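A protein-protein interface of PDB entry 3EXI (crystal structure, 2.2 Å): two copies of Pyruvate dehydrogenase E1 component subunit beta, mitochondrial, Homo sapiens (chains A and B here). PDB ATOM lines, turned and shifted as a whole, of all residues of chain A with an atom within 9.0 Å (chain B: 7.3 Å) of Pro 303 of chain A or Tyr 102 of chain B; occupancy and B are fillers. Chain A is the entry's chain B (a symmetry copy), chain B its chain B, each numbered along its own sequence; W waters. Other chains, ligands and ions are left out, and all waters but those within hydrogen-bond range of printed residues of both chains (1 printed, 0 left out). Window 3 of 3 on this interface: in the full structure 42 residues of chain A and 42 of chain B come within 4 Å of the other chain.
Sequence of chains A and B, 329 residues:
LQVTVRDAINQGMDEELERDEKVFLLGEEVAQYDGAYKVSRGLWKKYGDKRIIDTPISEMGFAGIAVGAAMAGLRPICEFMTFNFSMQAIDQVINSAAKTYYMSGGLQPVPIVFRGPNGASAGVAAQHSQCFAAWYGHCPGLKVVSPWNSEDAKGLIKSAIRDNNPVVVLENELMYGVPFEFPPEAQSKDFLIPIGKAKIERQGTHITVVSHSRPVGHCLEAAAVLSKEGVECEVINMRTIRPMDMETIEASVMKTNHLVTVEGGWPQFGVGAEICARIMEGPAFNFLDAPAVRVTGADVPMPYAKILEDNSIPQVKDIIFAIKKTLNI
O of Ala 126 of chain A is in hydrogen-bond range of NZ of Lys 99 of chain B (2.7 Å).
The indole nitrogen (NE1) of Trp 266 of chain A lies within hydrogen-bond range of the backbone carbonyl oxygen (O) of Val 300 of chain A, 2.8 Å away.
N of Ala 126 of chain A is in hydrogen-bond range of O of Met 302 of chain A (3.0 Å).
Ala 126 of chain A touches Met 103 of chain B.
Met 103 of chain B touches Gln 127 of chain A.
Trp 266 of chain A touches Lys 99 of chain B (CH2 to CE, 3.9 Å).
CD of Pro 140 of chain B touches CD2 of Trp 266 of chain A (3.3 Å).
Asp 299 of chain A touches Pro 140 of chain B.
Pro 140 of chain B touches Val 300 of chain A.
Tyr 102 of chain B touches Pro 301 of chain A.
Pro 301 of chain A touches Pro 140 of chain B (N to CB, 3.8 Å).
OH of Tyr 102 of chain B touches CB of Pro 303 of chain A, at 3.4 Å.
Pro 303 of chain A touches just one residue of chain B: Tyr 102.
Printed residues of chain A within 4 Å of Tyr 102 of chain B: Pro 301 (3.1 Å) and Pro 303 (3.4 Å).
Of the printed residues of chain B, Asp 299 of chain A touches Pro 140.
Printed residues of chain B within 4 Å of Ala 126 of chain A: Lys 99 (2.7 Å) and Met 103 (3.5 Å).
Of the printed residues of chain A, Lys 99 of chain B touches Ala 126 and Trp 266.
Ala 122 of chain A touches none of the printed residues of chain B.
Ala 298 of chain A touches none of the printed residues of chain B.
The nearest printed residue of chain B that does not touch Pro 301 of chain A is Lys 99 of chain B (4.2 Å).
Hydrophobic or aromatic side chains of chain B within 4 Å of the printed part of chain A: Tyr 102, Met 103 and Pro 140.
Printed residues of chain A that touch a printed residue of chain B: Ala 126, Gln 127, Trp 266, Asp 299, Val 300, Pro 301 and Pro 303.
Among the printed residues, 10 pairs touch across the chains.
Among the printed residues, no Asp or Glu carboxylate lies within 4 Å of a Lys or Arg side-chain nitrogen of the other chain.
No position is printed for both chains.
Water W1 bridges the backbone carbonyl oxygen of Gln 127 of chain A (3.3 Å) and the side-chain amino group of Lys 99 of chain B (3.3 Å).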
ATOM      1  N   ALA A 120      13.051  12.032  -7.846  1.00  0.00           N
ATOM      2  CA  ALA A 120      14.078  12.772  -8.537  1.00  0.00           C
ATOM      3  C   ALA A 120      15.207  11.862  -8.985  1.00  0.00           C
ATOM      4  O   ALA A 120      15.538  10.854  -8.344  1.00  0.00           O
ATOM      5  CB  ALA A 120      14.666  13.877  -7.638  1.00  0.00           C
ATOM      6  N   SER A 121      15.744  12.240 -10.135  1.00  0.00           N
ATOM      7  CA  SER A 121      16.896  11.616 -10.702  1.00  0.00           C
ATOM      8  C   SER A 121      17.879  12.798 -10.990  1.00  0.00           C
ATOM      9  O   SER A 121      18.058  13.689 -10.141  1.00  0.00           O
ATOM     10  CB  SER A 121      16.503  10.896 -11.985  1.00  0.00           C
ATOM     11  OG  SER A 121      17.561  10.155 -12.515  1.00  0.00           O
ATOM     12  N   ALA A 122      18.536  12.796 -12.149  1.00  0.00           N
ATOM     13  CA  ALA A 122      19.516  13.844 -12.440  1.00  0.00           C
ATOM     14  C   ALA A 122      19.295  14.407 -13.847  1.00  0.00           C
ATOM     15  O   ALA A 122      19.656  13.788 -14.834  1.00  0.00           O
ATOM     16  CB  ALA A 122      20.919  13.314 -12.286  1.00  0.00           C
ATOM     17  N   GLY A 123      18.646  15.556 -13.936  1.00  0.00           N
ATOM     18  CA  GLY A 123      18.549  16.227 -15.214  1.00  0.00           C
ATOM     19  C   GLY A 123      17.496  15.681 -16.168  1.00  0.00           C
ATOM     20  O   GLY A 123      17.556  15.959 -17.373  1.00  0.00           O
ATOM     21  N   VAL A 124      16.527  14.924 -15.662  1.00  0.00           N
ATOM     22  CA  VAL A 124      15.514  14.311 -16.542  1.00  0.00           C
ATOM     23  C   VAL A 124      14.216  15.184 -16.644  1.00  0.00           C
ATOM     24  O   VAL A 124      13.249  14.790 -17.325  1.00  0.00           O
ATOM     25  CB  VAL A 124      15.196  12.913 -16.116  1.00  0.00           C
ATOM     26  CG1 VAL A 124      16.474  12.002 -16.244  1.00  0.00           C
ATOM     27  CG2 VAL A 124      14.677  12.905 -14.696  1.00  0.00           C
ATOM     28  N   ALA A 125      14.211  16.314 -15.926  1.00  0.00           N
ATOM     29  CA  ALA A 125      13.166  17.335 -16.010  1.00  0.00           C
ATOM     30  C   ALA A 125      11.793  16.892 -15.457  1.00  0.00           C
ATOM     31  O   ALA A 125      11.705  15.851 -14.828  1.00  0.00           O
ATOM     32  CB  ALA A 125      13.046  17.862 -17.462  1.00  0.00           C
ATOM     33  N   ALA A 126      10.739  17.704 -15.676  1.00  0.00           N
ATOM     34  CA  ALA A 126       9.502  17.695 -14.850  1.00  0.00           C
ATOM     35  C   ALA A 126       8.634  16.437 -14.985  1.00  0.00           C
ATOM     36  O   ALA A 126       8.035  15.983 -13.978  1.00  0.00           O
ATOM     37  CB  ALA A 126       8.659  19.007 -15.128  1.00  0.00           C
ATOM     38  N   GLN A 127       8.579  15.880 -16.214  1.00  0.00           N
ATOM     39  CA  GLN A 127       7.806  14.665 -16.548  1.00  0.00           C
ATOM     40  C   GLN A 127       8.464  13.333 -16.052  1.00  0.00           C
ATOM     41  O   GLN A 127       7.850  12.247 -16.076  1.00  0.00           O
ATOM     42  CB  GLN A 127       7.568  14.641 -18.072  1.00  0.00           C
ATOM     43  CG  GLN A 127       6.530  15.692 -18.514  1.00  0.00           C
ATOM     44  CD  GLN A 127       6.199  15.564 -19.972  1.00  0.00           C
ATOM     45  OE1 GLN A 127       6.985  15.000 -20.720  1.00  0.00           O
ATOM     46  NE2 GLN A 127       5.065  16.124 -20.403  1.00  0.00           N
ATOM     47  N   SER A 129      10.474  13.166 -12.975  1.00  0.00           N
ATOM     48  CA  SER A 129      11.067  13.375 -11.642  1.00  0.00           C
ATOM     49  C   SER A 129      10.077  13.297 -10.482  1.00  0.00           C
ATOM     50  O   SER A 129      10.426  13.715  -9.364  1.00  0.00           O
ATOM     51  CB  SER A 129      11.732  14.760 -11.533  1.00  0.00           C
ATOM     52  OG  SER A 129      12.723  15.013 -12.509  1.00  0.00           O
ATOM     53  N   TRP A 266       6.706  16.526  -3.434  1.00  0.00           N
ATOM     54  CA  TRP A 266       6.151  17.874  -3.267  1.00  0.00           C
ATOM     55  C   TRP A 266       5.559  18.076  -1.873  1.00  0.00           C
ATOM     56  O   TRP A 266       4.993  17.168  -1.304  1.00  0.00           O
ATOM     57  CB  TRP A 266       5.058  18.097  -4.319  1.00  0.00           C
ATOM     58  CG  TRP A 266       5.579  18.240  -5.753  1.00  0.00           C
ATOM     59  CD1 TRP A 266       6.673  18.958  -6.169  1.00  0.00           C
ATOM     60  CD2 TRP A 266       5.017  17.634  -6.949  1.00  0.00           C
ATOM     61  NE1 TRP A 266       6.810  18.853  -7.549  1.00  0.00           N
ATOM     62  CE2 TRP A 266       5.814  18.042  -8.040  1.00  0.00           C
ATOM     63  CE3 TRP A 266       3.911  16.785  -7.192  1.00  0.00           C
ATOM     64  CZ2 TRP A 266       5.516  17.678  -9.356  1.00  0.00           C
ATOM     65  CZ3 TRP A 266       3.619  16.420  -8.501  1.00  0.00           C
ATOM     66  CH2 TRP A 266       4.400  16.888  -9.568  1.00  0.00           C
ATOM     67  N   ALA A 298      11.063  21.505  -3.509  1.00  0.00           N
ATOM     68  CA  ALA A 298      10.381  22.726  -3.862  1.00  0.00           C
ATOM     69  C   ALA A 298       9.055  22.423  -4.549  1.00  0.00           C
ATOM     70  O   ALA A 298       8.893  21.399  -5.212  1.00  0.00           O
ATOM     71  CB  ALA A 298      11.313  23.635  -4.761  1.00  0.00           C
ATOM     72  N   ASP A 299       8.134  23.348  -4.420  1.00  0.00           N
ATOM     73  CA  ASP A 299       6.757  23.167  -4.871  1.00  0.00           C
ATOM     74  C   ASP A 299       6.634  23.613  -6.341  1.00  0.00           C
ATOM     75  O   ASP A 299       5.810  24.489  -6.724  1.00  0.00           O
ATOM     76  CB  ASP A 299       5.852  23.957  -3.923  1.00  0.00           C
ATOM     77  CG  ASP A 299       4.430  23.422  -3.884  1.00  0.00           C
ATOM     78  OD1 ASP A 299       4.177  22.264  -4.325  1.00  0.00           O
ATOM     79  OD2 ASP A 299       3.546  24.187  -3.446  1.00  0.00           O
ATOM     80  N   VAL A 300       7.464  22.964  -7.169  1.00  0.00           N
ATOM     81  CA  VAL A 300       7.502  23.217  -8.629  1.00  0.00           C
ATOM     82  C   VAL A 300       7.586  21.917  -9.428  1.00  0.00           C
ATOM     83  O   VAL A 300       8.154  20.900  -8.947  1.00  0.00           O
ATOM     84  CB  VAL A 300       8.743  24.091  -9.039  1.00  0.00           C
ATOM     85  CG1 VAL A 300       8.595  25.525  -8.619  1.00  0.00           C
ATOM     86  CG2 VAL A 300      10.045  23.474  -8.440  1.00  0.00           C
ATOM     87  N   PRO A 301       7.132  21.970 -10.698  1.00  0.00           N
ATOM     88  CA  PRO A 301       7.591  20.913 -11.601  1.00  0.00           C
ATOM     89  C   PRO A 301       9.119  20.937 -11.608  1.00  0.00           C
ATOM     90  O   PRO A 301       9.724  22.038 -11.522  1.00  0.00           O
ATOM     91  CB  PRO A 301       7.049  21.387 -12.962  1.00  0.00           C
ATOM     92  CG  PRO A 301       5.873  22.397 -12.597  1.00  0.00           C
ATOM     93  CD  PRO A 301       6.473  23.079 -11.442  1.00  0.00           C
ATOM     94  N   MET A 302       9.761  19.785 -11.703  1.00  0.00           N
ATOM     95  CA  MET A 302      11.202  19.764 -11.660  1.00  0.00           C
ATOM     96  C   MET A 302      11.851  20.457 -12.851  1.00  0.00           C
ATOM     97  O   MET A 302      11.621  20.052 -14.003  1.00  0.00           O
ATOM     98  CB  MET A 302      11.671  18.313 -11.556  1.00  0.00           C
ATOM     99  CG  MET A 302      13.168  18.155 -11.298  1.00  0.00           C
ATOM    100  SD  MET A 302      13.661  18.860  -9.719  1.00  0.00           S
ATOM    101  CE  MET A 302      13.290  17.514  -8.649  1.00  0.00           C
ATOM    102  N   PRO A 303      12.675  21.527 -12.599  1.00  0.00           N
ATOM    103  CA  PRO A 303      13.375  22.190 -13.692  1.00  0.00           C
ATOM    104  C   PRO A 303      14.616  21.384 -14.118  1.00  0.00           C
ATOM    105  O   PRO A 303      15.123  20.546 -13.359  1.00  0.00           O
ATOM    106  CB  PRO A 303      13.803  23.555 -13.083  1.00  0.00           C
ATOM    107  CG  PRO A 303      14.002  23.221 -11.638  1.00  0.00           C
ATOM    108  CD  PRO A 303      13.011  22.131 -11.277  1.00  0.00           C
ATOM    109  N   TYR A 304      15.080  21.664 -15.332  1.00  0.00           N
ATOM    110  CA  TYR A 304      16.172  20.938 -15.910  1.00  0.00           C
ATOM    111  C   TYR A 304      17.523  21.466 -15.415  1.00  0.00           C
ATOM    112  O   TYR A 304      18.365  20.681 -14.943  1.00  0.00           O
ATOM    113  CB  TYR A 304      16.104  21.104 -17.419  1.00  0.00           C
ATOM    114  CG  TYR A 304      17.332  20.578 -18.118  1.00  0.00           C
ATOM    115  CD1 TYR A 304      17.659  19.227 -18.038  1.00  0.00           C
ATOM    116  CD2 TYR A 304      18.175  21.433 -18.840  1.00  0.00           C
ATOM    117  CE1 TYR A 304      18.767  18.712 -18.702  1.00  0.00           C
ATOM    118  CE2 TYR A 304      19.303  20.931 -19.511  1.00  0.00           C
ATOM    119  CZ  TYR A 304      19.596  19.561 -19.438  1.00  0.00           C
ATOM    120  OH  TYR A 304      20.693  19.019 -20.112  1.00  0.00           O
ATOM    121  N   ALA A 305      17.732  22.782 -15.554  1.00  0.00           N
ATOM    122  CA  ALA A 305      19.039  23.415 -15.231  1.00  0.00           C
ATOM    123  C   ALA A 305      19.500  22.939 -13.877  1.00  0.00           C
ATOM    124  O   ALA A 305      18.731  22.888 -12.907  1.00  0.00           O
ATOM    125  CB  ALA A 305      18.976  24.937 -15.255  1.00  0.00           C
ATOM    126  N   LYS A 306      20.767  22.588 -13.832  1.00  0.00           N
ATOM    127  CA  LYS A 306      21.334  21.915 -12.714  1.00  0.00           C
ATOM    128  C   LYS A 306      21.198  22.734 -11.436  1.00  0.00           C
ATOM    129  O   LYS A 306      20.728  22.237 -10.421  1.00  0.00           O
ATOM    130  CB  LYS A 306      22.800  21.635 -13.019  1.00  0.00           C
ATOM    131  CG  LYS A 306      23.589  21.325 -11.824  1.00  0.00           C
ATOM    132  CD  LYS A 306      23.461  19.906 -11.425  1.00  0.00           C
ATOM    133  CE  LYS A 306      24.792  19.461 -10.830  1.00  0.00           C
ATOM    134  NZ  LYS A 306      24.569  18.473  -9.707  1.00  0.00           N
ATOM    135  N   ILE A 307      21.604  23.985 -11.471  1.00  0.00           N
ATOM    136  CA  ILE A 307      21.413  24.808 -10.309  1.00  0.00           C
ATOM    137  C   ILE A 307      19.981  24.786  -9.805  1.00  0.00           C
ATOM    138  O   ILE A 307      19.765  24.684  -8.598  1.00  0.00           O
ATOM    139  CB  ILE A 307      21.905  26.272 -10.485  1.00  0.00           C
ATOM    140  CG1 ILE A 307      21.909  26.953  -9.108  1.00  0.00           C
ATOM    141  CG2 ILE A 307      21.080  27.082 -11.561  1.00  0.00           C
ATOM    142  CD1 ILE A 307      22.741  28.186  -9.079  1.00  0.00           C
ATOM    143  N   LEU A 308      19.020  24.891 -10.717  1.00  0.00           N
ATOM    144  CA  LEU A 308      17.587  24.904 -10.357  1.00  0.00           C
ATOM    145  C   LEU A 308      17.177  23.567  -9.743  1.00  0.00           C
ATOM    146  O   LEU A 308      16.480  23.511  -8.734  1.00  0.00           O
ATOM    147  CB  LEU A 308      16.723  25.180 -11.599  1.00  0.00           C
ATOM    148  CG  LEU A 308      17.034  26.503 -12.282  1.00  0.00           C
ATOM    149  CD1 LEU A 308      16.041  26.678 -13.418  1.00  0.00           C
ATOM    150  CD2 LEU A 308      16.877  27.636 -11.303  1.00  0.00           C
ATOM    151  N   GLU A 309      17.622  22.476 -10.364  1.00  0.00           N
ATOM    152  CA  GLU A 309      17.311  21.155  -9.887  1.00  0.00           C
ATOM    153  C   GLU A 309      17.866  20.927  -8.472  1.00  0.00           C
ATOM    154  O   GLU A 309      17.139  20.429  -7.578  1.00  0.00           O
ATOM    155  CB  GLU A 309      17.836  20.089 -10.851  1.00  0.00           C
ATOM    156  CG  GLU A 309      17.484  18.683 -10.398  1.00  0.00           C
ATOM    157  CD  GLU A 309      17.962  17.624 -11.324  1.00  0.00           C
ATOM    158  OE1 GLU A 309      17.141  16.835 -11.767  1.00  0.00           O
ATOM    159  OE2 GLU A 309      19.165  17.586 -11.628  1.00  0.00           O
ATOM    160  N   ASP A 310      19.157  21.253  -8.290  1.00  0.00           N
ATOM    161  CA  ASP A 310      19.828  21.174  -6.966  1.00  0.00           C
ATOM    162  C   ASP A 310      19.005  21.897  -5.850  1.00  0.00           C
ATOM    163  O   ASP A 310      18.980  21.493  -4.689  1.00  0.00           O
ATOM    164  CB  ASP A 310      21.217  21.814  -7.074  1.00  0.00           C
ATOM    165  CG  ASP A 310      22.237  20.902  -7.730  1.00  0.00           C
ATOM    166  OD1 ASP A 310      21.907  19.739  -7.976  1.00  0.00           O
ATOM    167  OD2 ASP A 310      23.362  21.353  -8.002  1.00  0.00           O
ATOM    168  N   ASN A 311      18.299  22.954  -6.234  1.00  0.00           N
ATOM    169  CA  ASN A 311      17.553  23.790  -5.303  1.00  0.00           C
ATOM    170  C   ASN A 311      16.069  23.456  -5.273  1.00  0.00           C
ATOM    171  O   ASN A 311      15.222  24.188  -4.661  1.00  0.00           O
ATOM    172  CB  ASN A 311      17.739  25.264  -5.680  1.00  0.00           C
ATOM    173  CG  ASN A 311      19.017  25.832  -5.105  1.00  0.00           C
ATOM    174  OD1 ASN A 311      19.059  26.185  -3.929  1.00  0.00           O
ATOM    175  ND2 ASN A 311      20.071  25.898  -5.914  1.00  0.00           N
ATOM    176  N   SER A 312      15.763  22.327  -5.890  1.00  0.00           N
ATOM    177  CA  SER A 312      14.406  21.842  -5.946  1.00  0.00           C
ATOM    178  C   SER A 312      14.256  20.566  -5.119  1.00  0.00           C
ATOM    179  O   SER A 312      13.154  20.053  -4.946  1.00  0.00           O
ATOM    180  CB  SER A 312      14.027  21.593  -7.414  1.00  0.00           C
ATOM    181  OG  SER A 312      13.820  22.820  -8.099  1.00  0.00           O
ATOM    182  N   ILE A 313      15.385  20.040  -4.657  1.00  0.00           N
ATOM    183  CA  ILE A 313      15.395  18.928  -3.750  1.00  0.00           C
ATOM    184  C   ILE A 313      16.049  19.315  -2.405  1.00  0.00           C
ATOM    185  O   ILE A 313      16.959  20.125  -2.344  1.00  0.00           O
ATOM    186  CB  ILE A 313      16.128  17.682  -4.361  1.00  0.00           C
ATOM    187  CG1 ILE A 313      17.612  17.848  -4.315  1.00  0.00           C
ATOM    188  CG2 ILE A 313      15.778  17.474  -5.833  1.00  0.00           C
ATOM    189  CD1 ILE A 313      18.319  16.574  -4.740  1.00  0.00           C
ATOM    190  N   ALA B  97      -0.770  18.846 -19.065  1.00  0.00           N
ATOM    191  CA  ALA B  97      -1.432  20.135 -18.818  1.00  0.00           C
ATOM    192  C   ALA B  97      -0.725  20.908 -17.710  1.00  0.00           C
ATOM    193  O   ALA B  97      -0.154  21.994 -17.949  1.00  0.00           O
ATOM    194  CB  ALA B  97      -2.931  19.971 -18.555  1.00  0.00           C
ATOM    195  N   ALA B  98      -0.642  20.309 -16.527  1.00  0.00           N
ATOM    196  CA  ALA B  98      -0.142  21.007 -15.355  1.00  0.00           C
ATOM    197  C   ALA B  98       1.256  21.565 -15.570  1.00  0.00           C
ATOM    198  O   ALA B  98       1.503  22.754 -15.283  1.00  0.00           O
ATOM    199  CB  ALA B  98      -0.165  20.060 -14.121  1.00  0.00           C
ATOM    200  N   LYS B  99       2.169  20.686 -16.033  1.00  0.00           N
ATOM    201  CA  LYS B  99       3.587  20.974 -16.041  1.00  0.00           C
ATOM    202  C   LYS B  99       4.085  21.828 -17.184  1.00  0.00           C
ATOM    203  O   LYS B  99       5.242  22.264 -17.172  1.00  0.00           O
ATOM    204  CB  LYS B  99       4.417  19.662 -16.022  1.00  0.00           C
ATOM    205  CG  LYS B  99       4.213  18.908 -14.729  1.00  0.00           C
ATOM    206  CD  LYS B  99       5.037  17.626 -14.687  1.00  0.00           C
ATOM    207  CE  LYS B  99       4.689  16.866 -13.429  1.00  0.00           C
ATOM    208  NZ  LYS B  99       5.447  15.543 -13.423  1.00  0.00           N
ATOM    209  N   THR B 100       3.215  22.092 -18.166  1.00  0.00           N
ATOM    210  CA  THR B 100       3.641  22.595 -19.479  1.00  0.00           C
ATOM    211  C   THR B 100       4.052  24.053 -19.524  1.00  0.00           C
ATOM    212  O   THR B 100       5.036  24.408 -20.141  1.00  0.00           O
ATOM    213  CB  THR B 100       2.577  22.279 -20.550  1.00  0.00           C
ATOM    214  OG1 THR B 100       2.648  20.870 -20.831  1.00  0.00           O
ATOM    215  CG2 THR B 100       2.810  23.075 -21.877  1.00  0.00           C
ATOM    216  N   TYR B 101       3.318  24.914 -18.866  1.00  0.00           N
ATOM    217  CA  TYR B 101       3.694  26.329 -18.865  1.00  0.00           C
ATOM    218  C   TYR B 101       5.089  26.491 -18.238  1.00  0.00           C
ATOM    219  O   TYR B 101       5.975  27.179 -18.780  1.00  0.00           O
ATOM    220  CB  TYR B 101       2.682  27.123 -18.091  1.00  0.00           C
ATOM    221  CG  TYR B 101       2.829  28.600 -18.324  1.00  0.00           C
ATOM    222  CD1 TYR B 101       2.503  29.160 -19.551  1.00  0.00           C
ATOM    223  CD2 TYR B 101       3.269  29.455 -17.290  1.00  0.00           C
ATOM    224  CE1 TYR B 101       2.621  30.545 -19.767  1.00  0.00           C
ATOM    225  CE2 TYR B 101       3.377  30.856 -17.491  1.00  0.00           C
ATOM    226  CZ  TYR B 101       3.064  31.380 -18.725  1.00  0.00           C
ATOM    227  OH  TYR B 101       3.161  32.729 -18.913  1.00  0.00           O
ATOM    228  N   TYR B 102       5.302  25.801 -17.131  1.00  0.00           N
ATOM    229  CA  TYR B 102       6.622  25.814 -16.476  1.00  0.00           C
ATOM    230  C   TYR B 102       7.726  25.299 -17.374  1.00  0.00           C
ATOM    231  O   TYR B 102       8.732  26.005 -17.605  1.00  0.00           O
ATOM    232  CB  TYR B 102       6.576  25.061 -15.160  1.00  0.00           C
ATOM    233  CG  TYR B 102       7.797  25.219 -14.292  1.00  0.00           C
ATOM    234  CD1 TYR B 102       7.918  26.272 -13.361  1.00  0.00           C
ATOM    235  CD2 TYR B 102       8.822  24.288 -14.356  1.00  0.00           C
ATOM    236  CE1 TYR B 102       9.062  26.376 -12.537  1.00  0.00           C
ATOM    237  CE2 TYR B 102       9.963  24.393 -13.550  1.00  0.00           C
ATOM    238  CZ  TYR B 102      10.067  25.441 -12.644  1.00  0.00           C
ATOM    239  OH  TYR B 102      11.232  25.497 -11.893  1.00  0.00           O
ATOM    240  N   MET B 103       7.568  24.074 -17.892  1.00  0.00           N
ATOM    241  CA  MET B 103       8.655  23.420 -18.673  1.00  0.00           C
ATOM    242  C   MET B 103       9.009  24.214 -19.936  1.00  0.00           C
ATOM    243  O   MET B 103      10.165  24.205 -20.404  1.00  0.00           O
ATOM    244  CB  MET B 103       8.213  22.008 -19.108  1.00  0.00           C
ATOM    245  CG  MET B 103       8.054  20.984 -17.978  1.00  0.00           C
ATOM    246  SD  MET B 103       7.791  19.277 -18.620  1.00  0.00           S
ATOM    247  CE  MET B 103       6.207  19.634 -19.461  1.00  0.00           C
ATOM    248  N   SER B 104       7.993  24.869 -20.504  1.00  0.00           N
ATOM    249  CA  SER B 104       8.161  25.682 -21.673  1.00  0.00           C
ATOM    250  C   SER B 104       8.721  27.090 -21.337  1.00  0.00           C
ATOM    251  O   SER B 104       8.845  27.913 -22.230  1.00  0.00           O
ATOM    252  CB  SER B 104       6.817  25.853 -22.419  1.00  0.00           C
ATOM    253  OG  SER B 104       5.928  26.686 -21.699  1.00  0.00           O
ATOM    254  N   GLY B 105       9.021  27.385 -20.066  1.00  0.00           N
ATOM    255  CA  GLY B 105       9.526  28.713 -19.721  1.00  0.00           C
ATOM    256  C   GLY B 105       8.529  29.848 -19.948  1.00  0.00           C
ATOM    257  O   GLY B 105       8.947  30.940 -20.259  1.00  0.00           O
ATOM    258  N   GLY B 106       7.233  29.585 -19.767  1.00  0.00           N
ATOM    259  CA  GLY B 106       6.199  30.583 -19.935  1.00  0.00           C
ATOM    260  C   GLY B 106       5.672  30.784 -21.357  1.00  0.00           C
ATOM    261  O   GLY B 106       4.927  31.732 -21.628  1.00  0.00           O
ATOM    262  N   LEU B 107       6.014  29.882 -22.266  1.00  0.00           N
ATOM    263  CA  LEU B 107       5.687  30.044 -23.681  1.00  0.00           C
ATOM    264  C   LEU B 107       4.328  29.384 -23.975  1.00  0.00           C
ATOM    265  O   LEU B 107       3.527  29.909 -24.787  1.00  0.00           O
ATOM    266  CB  LEU B 107       6.758  29.336 -24.471  1.00  0.00           C
ATOM    267  CG  LEU B 107       7.549  29.864 -25.653  1.00  0.00           C
ATOM    268  CD1 LEU B 107       9.030  29.322 -25.458  1.00  0.00           C
ATOM    269  CD2 LEU B 107       6.906  29.457 -27.035  1.00  0.00           C
ATOM    270  N   GLN B 108       4.069  28.230 -23.320  1.00  0.00           N
ATOM    271  CA  GLN B 108       2.869  27.441 -23.667  1.00  0.00           C
ATOM    272  C   GLN B 108       1.826  27.355 -22.536  1.00  0.00           C
ATOM    273  O   GLN B 108       1.961  26.520 -21.674  1.00  0.00           O
ATOM    274  CB  GLN B 108       3.266  26.032 -24.141  1.00  0.00           C
ATOM    275  CG  GLN B 108       2.065  25.177 -24.641  1.00  0.00           C
ATOM    276  CD  GLN B 108       1.323  25.721 -25.873  1.00  0.00           C
ATOM    277  OE1 GLN B 108       1.799  25.550 -26.983  1.00  0.00           O
ATOM    278  NE2 GLN B 108       0.147  26.323 -25.684  1.00  0.00           N
ATOM    279  N   PRO B 140       1.943  20.876  -8.451  1.00  0.00           N
ATOM    280  CA  PRO B 140       2.305  22.205  -8.973  1.00  0.00           C
ATOM    281  C   PRO B 140       1.831  22.379 -10.424  1.00  0.00           C
ATOM    282  O   PRO B 140       2.006  21.464 -11.258  1.00  0.00           O
ATOM    283  CB  PRO B 140       3.844  22.196  -8.902  1.00  0.00           C
ATOM    284  CG  PRO B 140       4.178  21.143  -7.825  1.00  0.00           C
ATOM    285  CD  PRO B 140       3.121  20.101  -7.976  1.00  0.00           C
ATOM    286  N   GLY B 141       1.252  23.533 -10.745  1.00  0.00           N
ATOM    287  CA  GLY B 141       0.808  23.816 -12.106  1.00  0.00           C
ATOM    288  C   GLY B 141      -0.686  23.664 -12.296  1.00  0.00           C
ATOM    289  O   GLY B 141      -1.280  24.169 -13.284  1.00  0.00           O
HETATM  290  O   HOH W   1       5.531  12.284 -13.792  1.00  0.00           O
